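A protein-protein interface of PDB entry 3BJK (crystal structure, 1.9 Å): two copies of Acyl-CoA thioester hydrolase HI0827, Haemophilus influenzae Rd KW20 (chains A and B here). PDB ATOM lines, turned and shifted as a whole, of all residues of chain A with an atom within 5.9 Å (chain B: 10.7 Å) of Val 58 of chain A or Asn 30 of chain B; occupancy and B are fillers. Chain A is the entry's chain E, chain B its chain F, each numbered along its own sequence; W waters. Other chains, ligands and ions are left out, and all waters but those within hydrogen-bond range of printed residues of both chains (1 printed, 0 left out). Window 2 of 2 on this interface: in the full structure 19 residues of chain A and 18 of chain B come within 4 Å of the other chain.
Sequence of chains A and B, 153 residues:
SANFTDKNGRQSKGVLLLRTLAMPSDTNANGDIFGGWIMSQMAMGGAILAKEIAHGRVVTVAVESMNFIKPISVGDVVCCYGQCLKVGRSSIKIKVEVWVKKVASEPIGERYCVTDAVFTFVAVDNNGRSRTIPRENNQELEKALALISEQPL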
ATOM      1  N   ALA A  47      10.865  28.416 -10.066  1.00  0.00           N
ATOM      2  CA  ALA A  47       9.445  28.183  -9.863  1.00  0.00           C
ATOM      3  C   ALA A  47       8.552  29.207 -10.580  1.00  0.00           C
ATOM      4  O   ALA A  47       7.432  28.866 -10.978  1.00  0.00           O
ATOM      5  CB  ALA A  47       9.106  28.108  -8.324  1.00  0.00           C
ATOM      6  N   ALA A  50       8.462  27.946 -14.062  1.00  0.00           N
ATOM      7  CA  ALA A  50       7.650  26.760 -14.032  1.00  0.00           C
ATOM      8  C   ALA A  50       6.152  27.077 -13.886  1.00  0.00           C
ATOM      9  O   ALA A  50       5.299  26.432 -14.545  1.00  0.00           O
ATOM     10  CB  ALA A  50       8.137  25.825 -12.949  1.00  0.00           C
ATOM     11  N   LYS A  51       5.817  28.013 -12.998  1.00  0.00           N
ATOM     12  CA  LYS A  51       4.451  28.431 -12.814  1.00  0.00           C
ATOM     13  C   LYS A  51       3.837  29.098 -14.075  1.00  0.00           C
ATOM     14  O   LYS A  51       2.663  28.909 -14.387  1.00  0.00           O
ATOM     15  CB  LYS A  51       4.327  29.369 -11.602  1.00  0.00           C
ATOM     16  CG  LYS A  51       4.528  28.751 -10.266  1.00  0.00           C
ATOM     17  CD  LYS A  51       4.509  29.804  -9.162  1.00  0.00           C
ATOM     18  CE  LYS A  51       5.615  29.593  -8.241  1.00  0.00           C
ATOM     19  NZ  LYS A  51       5.643  30.543  -7.098  1.00  0.00           N
ATOM     20  N   ALA A  54       3.181  26.283 -16.365  1.00  0.00           N
ATOM     21  CA  ALA A  54       2.202  25.326 -15.811  1.00  0.00           C
ATOM     22  C   ALA A  54       0.799  25.896 -15.665  1.00  0.00           C
ATOM     23  O   ALA A  54      -0.157  25.157 -15.348  1.00  0.00           O
ATOM     24  CB  ALA A  54       2.677  24.762 -14.514  1.00  0.00           C
ATOM     25  N   GLY A  56      -0.141  27.651 -13.343  1.00  0.00           N
ATOM     26  CA  GLY A  56      -0.551  27.635 -11.949  1.00  0.00           C
ATOM     27  C   GLY A  56       0.526  27.161 -11.010  1.00  0.00           C
ATOM     28  O   GLY A  56       1.727  27.281 -11.330  1.00  0.00           O
ATOM     29  N   ARG A  57       0.071  26.629  -9.858  1.00  0.00           N
ATOM     30  CA  ARG A  57       0.953  26.187  -8.759  1.00  0.00           C
ATOM     31  C   ARG A  57       1.882  25.058  -9.171  1.00  0.00           C
ATOM     32  O   ARG A  57       1.503  24.160  -9.941  1.00  0.00           O
ATOM     33  CB  ARG A  57       0.152  25.686  -7.568  1.00  0.00           C
ATOM     34  CG  ARG A  57      -0.749  26.717  -6.857  1.00  0.00           C
ATOM     35  CD  ARG A  57      -1.175  26.130  -5.552  1.00  0.00           C
ATOM     36  NE  ARG A  57      -2.097  26.924  -4.762  1.00  0.00           N
ATOM     37  CZ  ARG A  57      -1.793  27.998  -4.022  1.00  0.00           C
ATOM     38  NH1 ARG A  57      -0.566  28.554  -4.010  1.00  0.00           N
ATOM     39  NH2 ARG A  57      -2.769  28.568  -3.317  1.00  0.00           N
ATOM     40  N   VAL A  58       3.095  25.119  -8.651  1.00  0.00           N
ATOM     41  CA  VAL A  58       4.077  24.047  -8.761  1.00  0.00           C
ATOM     42  C   VAL A  58       4.772  23.774  -7.429  1.00  0.00           C
ATOM     43  O   VAL A  58       4.714  24.580  -6.489  1.00  0.00           O
ATOM     44  CB  VAL A  58       5.196  24.337  -9.822  1.00  0.00           C
ATOM     45  CG1 VAL A  58       4.584  24.685 -11.179  1.00  0.00           C
ATOM     46  CG2 VAL A  58       6.182  25.370  -9.344  1.00  0.00           C
ATOM     47  N   VAL A  59       5.443  22.629  -7.365  1.00  0.00           N
ATOM     48  CA  VAL A  59       6.342  22.275  -6.252  1.00  0.00           C
ATOM     49  C   VAL A  59       7.678  21.883  -6.830  1.00  0.00           C
ATOM     50  O   VAL A  59       7.716  21.406  -7.963  1.00  0.00           O
ATOM     51  CB  VAL A  59       5.785  21.097  -5.418  1.00  0.00           C
ATOM     52  CG1 VAL A  59       4.472  21.508  -4.735  1.00  0.00           C
ATOM     53  CG2 VAL A  59       5.558  19.831  -6.282  1.00  0.00           C
ATOM     54  N   THR A  60       8.759  22.071  -6.056  1.00  0.00           N
ATOM     55  CA  THR A  60      10.088  21.617  -6.466  1.00  0.00           C
ATOM     56  C   THR A  60      10.173  20.167  -6.071  1.00  0.00           C
ATOM     57  O   THR A  60       9.830  19.799  -4.941  1.00  0.00           O
ATOM     58  CB  THR A  60      11.250  22.362  -5.798  1.00  0.00           C
ATOM     59  OG1 THR A  60      11.088  23.784  -5.951  1.00  0.00           O
ATOM     60  CG2 THR A  60      12.559  21.929  -6.383  1.00  0.00           C
ATOM     61  N   ILE A  92       8.449  19.942 -15.216  1.00  0.00           N
ATOM     62  CA  ILE A  92       9.141  21.027 -15.912  1.00  0.00           C
ATOM     63  C   ILE A  92      10.570  21.075 -15.413  1.00  0.00           C
ATOM     64  O   ILE A  92      10.812  21.361 -14.241  1.00  0.00           O
ATOM     65  CB  ILE A  92       8.517  22.401 -15.615  1.00  0.00           C
ATOM     66  CG1 ILE A  92       7.029  22.394 -15.960  1.00  0.00           C
ATOM     67  CG2 ILE A  92       9.253  23.501 -16.415  1.00  0.00           C
ATOM     68  CD1 ILE A  92       6.220  23.175 -15.051  1.00  0.00           C
ATOM     69  N   PHE A 121      10.422  20.882 -11.447  1.00  0.00           N
ATOM     70  CA  PHE A 121       9.167  21.246 -10.812  1.00  0.00           C
ATOM     71  C   PHE A 121       8.038  20.389 -11.358  1.00  0.00           C
ATOM     72  O   PHE A 121       8.113  19.906 -12.466  1.00  0.00           O
ATOM     73  CB  PHE A 121       8.858  22.728 -11.047  1.00  0.00           C
ATOM     74  CG  PHE A 121       9.961  23.631 -10.623  1.00  0.00           C
ATOM     75  CD1 PHE A 121      10.980  23.968 -11.512  1.00  0.00           C
ATOM     76  CD2 PHE A 121       9.994  24.155  -9.316  1.00  0.00           C
ATOM     77  CE1 PHE A 121      11.992  24.794 -11.094  1.00  0.00           C
ATOM     78  CE2 PHE A 121      11.027  24.961  -8.902  1.00  0.00           C
ATOM     79  CZ  PHE A 121      12.014  25.262  -9.782  1.00  0.00           C
ATOM     80  N   VAL A 122       7.016  20.199 -10.537  1.00  0.00           N
ATOM     81  CA  VAL A 122       5.812  19.444 -10.880  1.00  0.00           C
ATOM     82  C   VAL A 122       4.600  20.368 -10.663  1.00  0.00           C
ATOM     83  O   VAL A 122       4.417  20.938  -9.568  1.00  0.00           O
ATOM     84  CB  VAL A 122       5.705  18.169 -10.055  1.00  0.00           C
ATOM     85  CG1 VAL A 122       4.311  17.529 -10.159  1.00  0.00           C
ATOM     86  CG2 VAL A 122       6.811  17.146 -10.464  1.00  0.00           C
ATOM     87  N   ALA A 123       3.772  20.481 -11.703  1.00  0.00           N
ATOM     88  CA  ALA A 123       2.490  21.159 -11.642  1.00  0.00           C
ATOM     89  C   ALA A 123       1.551  20.450 -10.656  1.00  0.00           C
ATOM     90  O   ALA A 123       1.262  19.277 -10.836  1.00  0.00           O
ATOM     91  CB  ALA A 123       1.838  21.196 -13.067  1.00  0.00           C
ATOM     92  N   VAL A 124       1.015  21.192  -9.680  1.00  0.00           N
ATOM     93  CA  VAL A 124       0.076  20.624  -8.702  1.00  0.00           C
ATOM     94  C   VAL A 124      -1.207  21.447  -8.544  1.00  0.00           C
ATOM     95  O   VAL A 124      -1.231  22.613  -8.858  1.00  0.00           O
ATOM     96  CB  VAL A 124       0.755  20.489  -7.302  1.00  0.00           C
ATOM     97  CG1 VAL A 124       1.893  19.477  -7.400  1.00  0.00           C
ATOM     98  CG2 VAL A 124       1.246  21.838  -6.783  1.00  0.00           C
ATOM     99  N   ARG A 131      -0.980  17.730 -11.489  1.00  0.00           N
ATOM    100  CA  ARG A 131      -1.984  17.972 -12.491  1.00  0.00           C
ATOM    101  C   ARG A 131      -1.306  18.111 -13.845  1.00  0.00           C
ATOM    102  O   ARG A 131      -0.107  18.426 -13.926  1.00  0.00           O
ATOM    103  CB  ARG A 131      -2.743  19.259 -12.151  1.00  0.00           C
ATOM    104  CG  ARG A 131      -1.865  20.487 -12.086  1.00  0.00           C
ATOM    105  CD  ARG A 131      -2.668  21.753 -11.770  1.00  0.00           C
ATOM    106  NE  ARG A 131      -1.702  22.821 -11.640  1.00  0.00           N
ATOM    107  CZ  ARG A 131      -1.261  23.570 -12.635  1.00  0.00           C
ATOM    108  NH1 ARG A 131      -1.773  23.494 -13.867  1.00  0.00           N
ATOM    109  NH2 ARG A 131      -0.311  24.419 -12.366  1.00  0.00           N
ATOM    110  N   PRO B  24       6.211  29.344  10.761  1.00  0.00           N
ATOM    111  CA  PRO B  24       5.431  30.090   9.767  1.00  0.00           C
ATOM    112  C   PRO B  24       6.188  31.045   8.833  1.00  0.00           C
ATOM    113  O   PRO B  24       5.835  31.124   7.646  1.00  0.00           O
ATOM    114  CB  PRO B  24       4.453  30.897  10.632  1.00  0.00           C
ATOM    115  CG  PRO B  24       4.304  30.070  11.861  1.00  0.00           C
ATOM    116  CD  PRO B  24       5.586  29.388  12.093  1.00  0.00           C
ATOM    117  N   ASP B  26       8.844  30.542   7.429  1.00  0.00           N
ATOM    118  CA  ASP B  26       9.539  29.810   6.358  1.00  0.00           C
ATOM    119  C   ASP B  26       8.666  29.110   5.401  1.00  0.00           C
ATOM    120  O   ASP B  26       9.095  28.192   4.737  1.00  0.00           O
ATOM    121  CB  ASP B  26      10.631  28.949   6.931  1.00  0.00           C
ATOM    122  CG  ASP B  26      11.703  29.821   7.645  1.00  0.00           C
ATOM    123  OD1 ASP B  26      12.318  30.765   6.994  1.00  0.00           O
ATOM    124  OD2 ASP B  26      11.840  29.573   8.848  1.00  0.00           O
ATOM    125  N   THR B  27       7.440  29.603   5.266  1.00  0.00           N
ATOM    126  CA  THR B  27       6.475  28.964   4.395  1.00  0.00           C
ATOM    127  C   THR B  27       6.566  29.582   2.977  1.00  0.00           C
ATOM    128  O   THR B  27       7.014  30.751   2.762  1.00  0.00           O
ATOM    129  CB  THR B  27       5.041  29.090   4.937  1.00  0.00           C
ATOM    130  OG1 THR B  27       4.787  30.452   5.282  1.00  0.00           O
ATOM    131  CG2 THR B  27       4.840  28.246   6.194  1.00  0.00           C
ATOM    132  N   ASN B  28       6.126  28.776   2.022  1.00  0.00           N
ATOM    133  CA  ASN B  28       5.963  29.207   0.664  1.00  0.00           C
ATOM    134  C   ASN B  28       4.527  29.702   0.395  1.00  0.00           C
ATOM    135  O   ASN B  28       3.695  29.743   1.289  1.00  0.00           O
ATOM    136  CB  ASN B  28       6.436  28.079  -0.286  1.00  0.00           C
ATOM    137  CG  ASN B  28       5.548  26.837  -0.248  1.00  0.00           C
ATOM    138  OD1 ASN B  28       4.407  26.884   0.230  1.00  0.00           O
ATOM    139  ND2 ASN B  28       6.069  25.705  -0.777  1.00  0.00           N
ATOM    140  N   ALA B  29       4.274  30.069  -0.856  1.00  0.00           N
ATOM    141  CA  ALA B  29       2.997  30.584  -1.280  1.00  0.00           C
ATOM    142  C   ALA B  29       1.983  29.434  -1.389  1.00  0.00           C
ATOM    143  O   ALA B  29       0.798  29.695  -1.458  1.00  0.00           O
ATOM    144  CB  ALA B  29       3.134  31.315  -2.602  1.00  0.00           C
ATOM    145  N   ASN B  30       2.435  28.174  -1.406  1.00  0.00           N
ATOM    146  CA  ASN B  30       1.473  27.053  -1.255  1.00  0.00           C
ATOM    147  C   ASN B  30       1.025  26.843   0.212  1.00  0.00           C
ATOM    148  O   ASN B  30       0.074  26.101   0.437  1.00  0.00           O
ATOM    149  CB  ASN B  30       2.041  25.724  -1.811  1.00  0.00           C
ATOM    150  CG  ASN B  30       2.444  25.795  -3.303  1.00  0.00           C
ATOM    151  OD1 ASN B  30       1.818  26.494  -4.103  1.00  0.00           O
ATOM    152  ND2 ASN B  30       3.450  25.009  -3.678  1.00  0.00           N
ATOM    153  N   GLY B  31       1.734  27.432   1.188  1.00  0.00           N
ATOM    154  CA  GLY B  31       1.466  27.244   2.638  1.00  0.00           C
ATOM    155  C   GLY B  31       2.289  26.131   3.321  1.00  0.00           C
ATOM    156  O   GLY B  31       2.237  25.925   4.542  1.00  0.00           O
ATOM    157  N   ASP B  32       3.027  25.385   2.501  1.00  0.00           N
ATOM    158  CA  ASP B  32       4.010  24.432   3.005  1.00  0.00           C
ATOM    159  C   ASP B  32       5.350  25.108   3.288  1.00  0.00           C
ATOM    160  O   ASP B  32       5.570  26.313   3.033  1.00  0.00           O
ATOM    161  CB  ASP B  32       4.179  23.316   1.980  1.00  0.00           C
ATOM    162  CG  ASP B  32       2.874  22.767   1.518  1.00  0.00           C
ATOM    163  OD1 ASP B  32       2.101  22.363   2.415  1.00  0.00           O
ATOM    164  OD2 ASP B  32       2.615  22.726   0.281  1.00  0.00           O
ATOM    165  N   ILE B  33       6.276  24.333   3.828  1.00  0.00           N
ATOM    166  CA  ILE B  33       7.601  24.889   4.065  1.00  0.00           C
ATOM    167  C   ILE B  33       8.386  25.006   2.739  1.00  0.00           C
ATOM    168  O   ILE B  33       8.431  24.086   1.912  1.00  0.00           O
ATOM    169  CB  ILE B  33       8.404  24.130   5.182  1.00  0.00           C
ATOM    170  CG1 ILE B  33       7.736  24.332   6.562  1.00  0.00           C
ATOM    171  CG2 ILE B  33       9.871  24.563   5.166  1.00  0.00           C
ATOM    172  CD1 ILE B  33       7.785  25.722   7.148  1.00  0.00           C
ATOM    173  N   PHE B  34       8.967  26.193   2.555  1.00  0.00           N
ATOM    174  CA  PHE B  34       9.744  26.556   1.358  1.00  0.00           C
ATOM    175  C   PHE B  34      10.951  25.632   1.127  1.00  0.00           C
ATOM    176  O   PHE B  34      11.758  25.437   2.034  1.00  0.00           O
ATOM    177  CB  PHE B  34      10.172  28.052   1.520  1.00  0.00           C
ATOM    178  CG  PHE B  34      11.032  28.612   0.387  1.00  0.00           C
ATOM    179  CD1 PHE B  34      10.758  28.328  -0.957  1.00  0.00           C
ATOM    180  CD2 PHE B  34      12.130  29.431   0.681  1.00  0.00           C
ATOM    181  CE1 PHE B  34      11.563  28.868  -1.997  1.00  0.00           C
ATOM    182  CE2 PHE B  34      12.931  29.998  -0.361  1.00  0.00           C
ATOM    183  CZ  PHE B  34      12.656  29.700  -1.694  1.00  0.00           C
ATOM    184  N   GLY B  35      11.094  25.117  -0.099  1.00  0.00           N
ATOM    185  CA  GLY B  35      12.224  24.264  -0.518  1.00  0.00           C
ATOM    186  C   GLY B  35      13.596  24.913  -0.259  1.00  0.00           C
ATOM    187  O   GLY B  35      14.525  24.207   0.114  1.00  0.00           O
ATOM    188  N   PHE B  68      13.079  16.019  -3.339  1.00  0.00           N
ATOM    189  CA  PHE B  68      12.083  16.499  -2.411  1.00  0.00           C
ATOM    190  C   PHE B  68      10.971  15.490  -2.465  1.00  0.00           C
ATOM    191  O   PHE B  68      10.300  15.349  -3.484  1.00  0.00           O
ATOM    192  CB  PHE B  68      11.607  17.892  -2.776  1.00  0.00           C
ATOM    193  CG  PHE B  68      12.695  18.944  -2.725  1.00  0.00           C
ATOM    194  CD1 PHE B  68      13.495  19.175  -3.839  1.00  0.00           C
ATOM    195  CD2 PHE B  68      12.911  19.696  -1.585  1.00  0.00           C
ATOM    196  CE1 PHE B  68      14.505  20.155  -3.821  1.00  0.00           C
ATOM    197  CE2 PHE B  68      13.911  20.660  -1.546  1.00  0.00           C
ATOM    198  CZ  PHE B  68      14.709  20.889  -2.678  1.00  0.00           C
ATOM    199  N   PRO B  71       6.275  16.972   1.489  1.00  0.00           N
ATOM    200  CA  PRO B  71       6.349  18.319   1.982  1.00  0.00           C
ATOM    201  C   PRO B  71       6.600  18.379   3.478  1.00  0.00           C
ATOM    202  O   PRO B  71       6.373  17.415   4.202  1.00  0.00           O
ATOM    203  CB  PRO B  71       4.975  18.928   1.636  1.00  0.00           C
ATOM    204  CG  PRO B  71       4.098  17.778   1.526  1.00  0.00           C
ATOM    205  CD  PRO B  71       4.918  16.612   1.061  1.00  0.00           C
ATOM    206  N   ILE B  72       7.113  19.518   3.892  1.00  0.00           N
ATOM    207  CA  ILE B  72       7.269  19.839   5.294  1.00  0.00           C
ATOM    208  C   ILE B  72       6.162  20.844   5.654  1.00  0.00           C
ATOM    209  O   ILE B  72       5.796  21.718   4.840  1.00  0.00           O
ATOM    210  CB  ILE B  72       8.678  20.378   5.590  1.00  0.00           C
ATOM    211  CG1 ILE B  72       9.723  19.351   5.134  1.00  0.00           C
ATOM    212  CG2 ILE B  72       8.809  20.702   7.077  1.00  0.00           C
ATOM    213  CD1 ILE B  72      11.121  19.655   5.596  1.00  0.00           C
ATOM    214  N   SER B  73       5.637  20.696   6.882  1.00  0.00           N
ATOM    215  CA  SER B  73       4.558  21.543   7.386  1.00  0.00           C
ATOM    216  C   SER B  73       5.019  22.331   8.582  1.00  0.00           C
ATOM    217  O   SER B  73       5.871  21.882   9.358  1.00  0.00           O
ATOM    218  CB  SER B  73       3.365  20.713   7.765  1.00  0.00           C
ATOM    219  OG  SER B  73       2.984  19.957   6.640  1.00  0.00           O
ATOM    220  N   VAL B  74       4.494  23.537   8.700  1.00  0.00           N
ATOM    221  CA  VAL B  74       4.674  24.331   9.949  1.00  0.00           C
ATOM    222  C   VAL B  74       4.391  23.488  11.179  1.00  0.00           C
ATOM    223  O   VAL B  74       3.343  22.766  11.244  1.00  0.00           O
ATOM    224  CB  VAL B  74       3.769  25.595   9.991  1.00  0.00           C
ATOM    225  CG1 VAL B  74       3.818  26.263  11.401  1.00  0.00           C
ATOM    226  CG2 VAL B  74       4.193  26.580   8.879  1.00  0.00           C
HETATM  227  O   HOH W   1      11.263  25.202  -3.428  1.00  0.00           O
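O of Ala 29 of chain B is in hydrogen-bond range of NH1 of Arg 57 of chain A.
OD1 of Asn 30 of chain B is in hydrogen-bond range of NH1 of Arg 57 of chain A (3.2 Å).
The backbone carbonyl oxygen (O) of Val 58 of chain A lies within hydrogen-bond range of the side-chain amide nitrogen (ND2) of Asn 30 of chain B, 3.1 Å away.
O of Arg 57 of chain A is in hydrogen-bond range of N of Val 124 of chain A (3.0 Å).
The backbone carbonyl oxygen of Arg 57 of chain A is in hydrogen-bond range of the guanidinium group of Arg 131 of chain A (3.0 Å).
The backbone carbonyl oxygen of Val 59 of chain A sits at hydrogen-bond distance from the backbone NH of Val 122 of chain A.
The backbone NH (N) of Asn 30 of chain B sits at hydrogen-bond distance from the side-chain amide oxygen (OD1) of Asn 28 of chain B, at 2.9 Å.
Of the 16 printed residues of chain B, 3 touch a printed residue of chain A.
Printed residues of chain B that touch a printed residue of chain A: Ala 29, Asn 30 and Phe 68.
Of the 15 printed residues of chain A, 4 touch a printed residue of chain B.
Hydrophobic or aromatic side chains of chain A that line the printed part of chain B: Val 59.
Among the printed residues, 5 pairs touch across the chains.
Among the printed residues, no Asp or Glu carboxylate lies within 4 Å of a Lys or Arg side-chain nitrogen of the other chain.
No position is printed for both chains.
Of the 5 pairs that touch across the chains among the printed residues, none has its exchanged pair printed and touching as well.
Water W1 bridges the side-chain hydroxyl (OG1) of Thr 60 of chain A (2.9 Å) and the backbone NH (N) of Gly 35 of chain B (3.3 Å).
Of chain B, only Asn 30 comes within 4 Å of Val 58 of chain A.
Asn 30 of chain B touches just these residues of chain A: Arg 57 (3.2 Å), Val 58 (3.1 Å) and Val 59 (3.8 Å).
Ala 47 of chain A touches none of the printed residues of chain B.
No residue of chain B comes within 4 Å of Ala 50 of chain A.
No residue of chain B comes within 4 Å of Lys 51 of chain A.
No residue of chain B comes within 4 Å of Ala 54 of chain A.
No residue of chain B comes within 4 Å of Gly 56 of chain A.
Arg 57 of chain A touches two residues of chain B.
No residue of chain B comes within 4 Å of Ala 123 of chain A.
No residue of chain B comes within 4 Å of Val 124 of chain A.
Of the printed residues of chain A, Phe 68 of chain B touches Thr 60.
Of the printed residues of chain A, Ala 29 of chain B touches Arg 57 (3.1 Å).
Of the printed residues of chain B, Thr 60 of chain A touches Phe 68.
Gly 31 of chain B touches none of the printed residues of chain A.
Phe 34 of chain B touches none of the printed residues of chain A.
Among the printed residues, merely in contact across the chains: Val 59 of chain A with Asn 30 of chain B (3.8 Å) and Thr 60 of chain A with Phe 68 of chain B (3.4 Å).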
